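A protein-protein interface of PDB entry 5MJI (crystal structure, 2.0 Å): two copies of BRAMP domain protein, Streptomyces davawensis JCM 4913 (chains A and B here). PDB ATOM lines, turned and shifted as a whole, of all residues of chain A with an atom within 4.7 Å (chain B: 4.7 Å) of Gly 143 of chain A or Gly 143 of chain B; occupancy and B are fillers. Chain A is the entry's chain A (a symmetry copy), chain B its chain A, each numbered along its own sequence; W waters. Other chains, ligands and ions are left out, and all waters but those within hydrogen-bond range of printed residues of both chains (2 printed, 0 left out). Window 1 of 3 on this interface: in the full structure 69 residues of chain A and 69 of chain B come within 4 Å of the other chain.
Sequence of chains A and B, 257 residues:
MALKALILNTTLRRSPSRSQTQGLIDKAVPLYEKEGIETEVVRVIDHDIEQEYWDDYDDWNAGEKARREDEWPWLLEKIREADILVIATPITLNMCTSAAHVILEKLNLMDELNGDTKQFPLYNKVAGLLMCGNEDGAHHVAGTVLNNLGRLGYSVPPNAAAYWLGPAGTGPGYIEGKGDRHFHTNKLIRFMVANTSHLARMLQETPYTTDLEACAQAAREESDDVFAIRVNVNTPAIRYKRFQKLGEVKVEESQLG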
ATOM      1  N   HIS A 139      14.175 -27.433   5.885  1.00  0.00           N
ATOM      2  CA  HIS A 139      12.847 -27.479   5.286  1.00  0.00           C
ATOM      3  C   HIS A 139      12.438 -26.126   4.726  1.00  0.00           C
ATOM      4  O   HIS A 139      11.776 -26.059   3.682  1.00  0.00           O
ATOM      5  CB  HIS A 139      11.829 -27.990   6.301  1.00  0.00           C
ATOM      6  CG  HIS A 139      11.973 -29.451   6.573  1.00  0.00           C
ATOM      7  ND1 HIS A 139      12.494 -29.946   7.745  1.00  0.00           N
ATOM      8  CD2 HIS A 139      11.743 -30.523   5.783  1.00  0.00           C
ATOM      9  CE1 HIS A 139      12.536 -31.264   7.684  1.00  0.00           C
ATOM     10  NE2 HIS A 139      12.093 -31.638   6.500  1.00  0.00           N
ATOM     11  N   HIS A 140      12.818 -25.041   5.404  1.00  0.00           N
ATOM     12  CA  HIS A 140      12.527 -23.710   4.891  1.00  0.00           C
ATOM     13  C   HIS A 140      13.219 -23.473   3.554  1.00  0.00           C
ATOM     14  O   HIS A 140      12.610 -22.962   2.607  1.00  0.00           O
ATOM     15  CB  HIS A 140      12.960 -22.657   5.904  1.00  0.00           C
ATOM     16  CG  HIS A 140      12.607 -21.263   5.498  1.00  0.00           C
ATOM     17  ND1 HIS A 140      13.252 -20.157   6.003  1.00  0.00           N
ATOM     18  CD2 HIS A 140      11.669 -20.795   4.640  1.00  0.00           C
ATOM     19  CE1 HIS A 140      12.733 -19.067   5.466  1.00  0.00           C
ATOM     20  NE2 HIS A 140      11.780 -19.427   4.626  1.00  0.00           N
ATOM     21  N   VAL A 141      14.495 -23.843   3.462  1.00  0.00           N
ATOM     22  CA  VAL A 141      15.227 -23.695   2.208  1.00  0.00           C
ATOM     23  C   VAL A 141      14.657 -24.617   1.135  1.00  0.00           C
ATOM     24  O   VAL A 141      14.543 -24.226  -0.034  1.00  0.00           O
ATOM     25  CB  VAL A 141      16.726 -23.944   2.442  1.00  0.00           C
ATOM     26  CG1 VAL A 141      17.493 -23.990   1.104  1.00  0.00           C
ATOM     27  CG2 VAL A 141      17.299 -22.821   3.316  1.00  0.00           C
ATOM     28  N   ALA A 142      14.285 -25.852   1.509  1.00  0.00           N
ATOM     29  CA  ALA A 142      13.679 -26.756   0.538  1.00  0.00           C
ATOM     30  C   ALA A 142      12.417 -26.150  -0.062  1.00  0.00           C
ATOM     31  O   ALA A 142      12.241 -26.147  -1.285  1.00  0.00           O
ATOM     32  CB  ALA A 142      13.376 -28.125   1.170  1.00  0.00           C
ATOM     33  N   GLY A 143      11.536 -25.614   0.782  1.00  0.00           N
ATOM     34  CA  GLY A 143      10.323 -24.991   0.272  1.00  0.00           C
ATOM     35  C   GLY A 143      10.617 -23.872  -0.715  1.00  0.00           C
ATOM     36  O   GLY A 143      10.053 -23.825  -1.811  1.00  0.00           O
ATOM     37  N   THR A 144      11.543 -22.984  -0.359  1.00  0.00           N
ATOM     38  CA  THR A 144      11.802 -21.809  -1.183  1.00  0.00           C
ATOM     39  C   THR A 144      12.449 -22.199  -2.505  1.00  0.00           C
ATOM     40  O   THR A 144      11.986 -21.793  -3.577  1.00  0.00           O
ATOM     41  CB  THR A 144      12.678 -20.816  -0.404  1.00  0.00           C
ATOM     42  OG1 THR A 144      12.014 -20.467   0.815  1.00  0.00           O
ATOM     43  CG2 THR A 144      12.948 -19.527  -1.222  1.00  0.00           C
ATOM     44  N   VAL A 145      13.500 -23.022  -2.453  1.00  0.00           N
ATOM     45  CA  VAL A 145      14.228 -23.377  -3.670  1.00  0.00           C
ATOM     46  C   VAL A 145      13.371 -24.247  -4.578  1.00  0.00           C
ATOM     47  O   VAL A 145      13.259 -23.984  -5.781  1.00  0.00           O
ATOM     48  CB  VAL A 145      15.563 -24.059  -3.315  1.00  0.00           C
ATOM     49  CG1 VAL A 145      16.271 -24.577  -4.582  1.00  0.00           C
ATOM     50  CG2 VAL A 145      16.455 -23.073  -2.545  1.00  0.00           C
ATOM     51  N   LEU A 146      12.742 -25.289  -4.021  1.00  0.00           N
ATOM     52  CA  LEU A 146      11.961 -26.192  -4.863  1.00  0.00           C
ATOM     53  C   LEU A 146      10.723 -25.509  -5.432  1.00  0.00           C
ATOM     54  O   LEU A 146      10.331 -25.806  -6.567  1.00  0.00           O
ATOM     55  CB  LEU A 146      11.569 -27.447  -4.091  1.00  0.00           C
ATOM     56  CG  LEU A 146      12.786 -28.351  -3.813  1.00  0.00           C
ATOM     57  CD1 LEU A 146      12.417 -29.479  -2.867  1.00  0.00           C
ATOM     58  CD2 LEU A 146      13.376 -28.916  -5.109  1.00  0.00           C
ATOM     59  N   ASN A 147      10.101 -24.596  -4.681  1.00  0.00           N
ATOM     60  CA  ASN A 147       9.005 -23.820  -5.258  1.00  0.00           C
ATOM     61  C   ASN A 147       9.494 -23.032  -6.472  1.00  0.00           C
ATOM     62  O   ASN A 147       8.862 -23.039  -7.534  1.00  0.00           O
ATOM     63  CB  ASN A 147       8.394 -22.872  -4.221  1.00  0.00           C
ATOM     64  CG  ASN A 147       7.305 -21.980  -4.828  1.00  0.00           C
ATOM     65  OD1 ASN A 147       7.509 -20.784  -5.034  1.00  0.00           O
ATOM     66  ND2 ASN A 147       6.167 -22.573  -5.149  1.00  0.00           N
ATOM     67  N   HIS B 139       3.625 -17.605  -2.675  1.00  0.00           N
ATOM     68  CA  HIS B 139       4.812 -18.422  -2.894  1.00  0.00           C
ATOM     69  C   HIS B 139       5.350 -18.989  -1.589  1.00  0.00           C
ATOM     70  O   HIS B 139       5.838 -20.127  -1.559  1.00  0.00           O
ATOM     71  CB  HIS B 139       5.878 -17.616  -3.629  1.00  0.00           C
ATOM     72  CG  HIS B 139       5.535 -17.382  -5.063  1.00  0.00           C
ATOM     73  ND1 HIS B 139       5.132 -16.159  -5.545  1.00  0.00           N
ATOM     74  CD2 HIS B 139       5.449 -18.241  -6.102  1.00  0.00           C
ATOM     75  CE1 HIS B 139       4.858 -16.264  -6.832  1.00  0.00           C
ATOM     76  NE2 HIS B 139       5.035 -17.520  -7.192  1.00  0.00           N
ATOM     77  N   HIS B 140       5.274 -18.214  -0.505  1.00  0.00           N
ATOM     78  CA  HIS B 140       5.700 -18.715   0.793  1.00  0.00           C
ATOM     79  C   HIS B 140       4.852 -19.905   1.228  1.00  0.00           C
ATOM     80  O   HIS B 140       5.379 -20.921   1.697  1.00  0.00           O
ATOM     81  CB  HIS B 140       5.621 -17.602   1.831  1.00  0.00           C
ATOM     82  CG  HIS B 140       6.135 -18.006   3.174  1.00  0.00           C
ATOM     83  ND1 HIS B 140       5.776 -17.356   4.334  1.00  0.00           N
ATOM     84  CD2 HIS B 140       6.988 -18.992   3.543  1.00  0.00           C
ATOM     85  CE1 HIS B 140       6.379 -17.929   5.360  1.00  0.00           C
ATOM     86  NE2 HIS B 140       7.110 -18.932   4.908  1.00  0.00           N
ATOM     87  N   VAL B 141       3.534 -19.794   1.075  1.00  0.00           N
ATOM     88  CA  VAL B 141       2.646 -20.899   1.423  1.00  0.00           C
ATOM     89  C   VAL B 141       2.871 -22.089   0.495  1.00  0.00           C
ATOM     90  O   VAL B 141       2.861 -23.244   0.941  1.00  0.00           O
ATOM     91  CB  VAL B 141       1.183 -20.424   1.402  1.00  0.00           C
ATOM     92  CG1 VAL B 141       0.216 -21.613   1.570  1.00  0.00           C
ATOM     93  CG2 VAL B 141       0.957 -19.421   2.541  1.00  0.00           C
ATOM     94  N   ALA B 142       3.083 -21.833  -0.805  1.00  0.00           N
ATOM     95  CA  ALA B 142       3.363 -22.928  -1.728  1.00  0.00           C
ATOM     96  C   ALA B 142       4.597 -23.708  -1.294  1.00  0.00           C
ATOM     97  O   ALA B 142       4.572 -24.942  -1.236  1.00  0.00           O
ATOM     98  CB  ALA B 142       3.528 -22.411  -3.167  1.00  0.00           C
ATOM     99  N   GLY B 143       5.680 -23.005  -0.964  1.00  0.00           N
ATOM    100  CA  GLY B 143       6.884 -23.689  -0.511  1.00  0.00           C
ATOM    101  C   GLY B 143       6.629 -24.566   0.705  1.00  0.00           C
ATOM    102  O   GLY B 143       7.010 -25.739   0.735  1.00  0.00           O
ATOM    103  N   THR B 144       5.936 -24.023   1.704  1.00  0.00           N
ATOM    104  CA  THR B 144       5.751 -24.744   2.958  1.00  0.00           C
ATOM    105  C   THR B 144       4.844 -25.952   2.768  1.00  0.00           C
ATOM    106  O   THR B 144       5.191 -27.070   3.165  1.00  0.00           O
ATOM    107  CB  THR B 144       5.193 -23.789   4.024  1.00  0.00           C
ATOM    108  OG1 THR B 144       6.094 -22.687   4.179  1.00  0.00           O
ATOM    109  CG2 THR B 144       5.018 -24.498   5.392  1.00  0.00           C
ATOM    110  N   VAL B 145       3.691 -25.755   2.122  1.00  0.00           N
ATOM    111  CA  VAL B 145       2.727 -26.844   1.972  1.00  0.00           C
ATOM    112  C   VAL B 145       3.267 -27.918   1.039  1.00  0.00           C
ATOM    113  O   VAL B 145       3.227 -29.111   1.361  1.00  0.00           O
ATOM    114  CB  VAL B 145       1.370 -26.295   1.490  1.00  0.00           C
ATOM    115  CG1 VAL B 145       0.391 -27.443   1.180  1.00  0.00           C
ATOM    116  CG2 VAL B 145       0.793 -25.346   2.553  1.00  0.00           C
ATOM    117  N   LEU B 146       3.792 -27.517  -0.126  1.00  0.00           N
ATOM    118  CA  LEU B 146       4.262 -28.515  -1.084  1.00  0.00           C
ATOM    119  C   LEU B 146       5.490 -29.258  -0.572  1.00  0.00           C
ATOM    120  O   LEU B 146       5.638 -30.454  -0.851  1.00  0.00           O
ATOM    121  CB  LEU B 146       4.555 -27.871  -2.435  1.00  0.00           C
ATOM    122  CG  LEU B 146       3.262 -27.427  -3.149  1.00  0.00           C
ATOM    123  CD1 LEU B 146       3.581 -26.603  -4.382  1.00  0.00           C
ATOM    124  CD2 LEU B 146       2.385 -28.625  -3.523  1.00  0.00           C
ATOM    125  N   ASN B 147       6.371 -28.588   0.176  1.00  0.00           N
ATOM    126  CA  ASN B 147       7.476 -29.311   0.803  1.00  0.00           C
ATOM    127  C   ASN B 147       6.939 -30.392   1.740  1.00  0.00           C
ATOM    128  O   ASN B 147       7.381 -31.545   1.703  1.00  0.00           O
ATOM    129  CB  ASN B 147       8.396 -28.356   1.569  1.00  0.00           C
ATOM    130  CG  ASN B 147       9.510 -29.102   2.313  1.00  0.00           C
ATOM    131  OD1 ASN B 147       9.481 -29.223   3.538  1.00  0.00           O
ATOM    132  ND2 ASN B 147      10.464 -29.635   1.569  1.00  0.00           N
HETATM  133  O   HOH W   1       8.657 -21.105   1.199  1.00  0.00           O
HETATM  134  O   HOH W   2       9.311 -22.903   2.986  1.00  0.00           O
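Printed residues of chain B within 4 Å of His 139 of chain A: Asn 147. Of chain B, only Gly 143 comes within 4 Å of Gly 143 of chain A. Of the printed residues of chain B, Asn 147 of chain A touches His 139 (3.4 Å) and Ala 142 (3.3 Å). Printed residues of chain A within 4 Å of His 139 of chain B: Asn 147 (3.4 Å). Printed residues of chain A within 4 Å of Ala 142 of chain B: Asn 147. Of chain A, only Gly 143 (3.4 Å) comes within 4 Å of Gly 143 of chain B. Of the printed residues of chain A, Asn 147 of chain B touches His 139 (3.4 Å) and Ala 142 (3.3 Å). The nearest residue of chain B that does not touch Gly 143 of chain A is Asn 147 of chain B (4.1 Å). The nearest printed residue of chain B that does not touch Ala 142 of chain A is Gly 143 of chain B (5.5 Å).
Of the 9 printed residues of chain B, 4 touch a printed residue of chain A. Hydrophobic or aromatic side chains of chain B within 4 Å of the printed part of chain A: His 139 and Ala 142. Of the 9 printed residues of chain A, 4 touch a printed residue of chain B. Hydrophobic or aromatic side chains of chain A within 4 Å of the printed part of chain B: His 139 and Ala 142. Among the printed residues, 5 pairs touch across the chains. Among the printed residues, no Asp or Glu carboxylate lies within 4 Å of a Lys or Arg side-chain nitrogen of the other chain.
His 139 of chain A touches Asn 147 of chain B (CD2 to OD1, 3.4 Å). CB of Ala 142 of chain A touches ND2 of Asn 147 of chain B, at 3.3 Å. Gly 143 of chain B touches Gly 143 of chain A. Asn 147 of chain A touches His 139 of chain B. Ala 142 of chain B touches Asn 147 of chain A (CB to ND2, 3.3 Å).
His 139 of chain A touches Asn 147 of chain B, and with the chains exchanged Asn 147 of chain A touches His 139 of chain B. Ala 142 of chain A touches Asn 147 of chain B, and with the chains exchanged Asn 147 of chain A touches Ala 142 of chain B. Gly 143 of chain B touches its own counterpart, Gly 143 of chain A. Positions printed for both chains: 139, 140, 141, 142, 143, 144, 145, 146 and 147. Of the 5 pairs that touch across the chains among the printed residues, 5 have their exchanged pair printed and touching as well.
Water W1 bridges O of His 140 of chain B (3.3 Å) and OG1 of Thr 144 of chain A (3.4 Å). Water W2 bridges the backbone carbonyl oxygen (O) of His 140 of chain A (3.3 Å) and the side-chain hydroxyl (OG1) of Thr 144 of chain B (3.4 Å).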
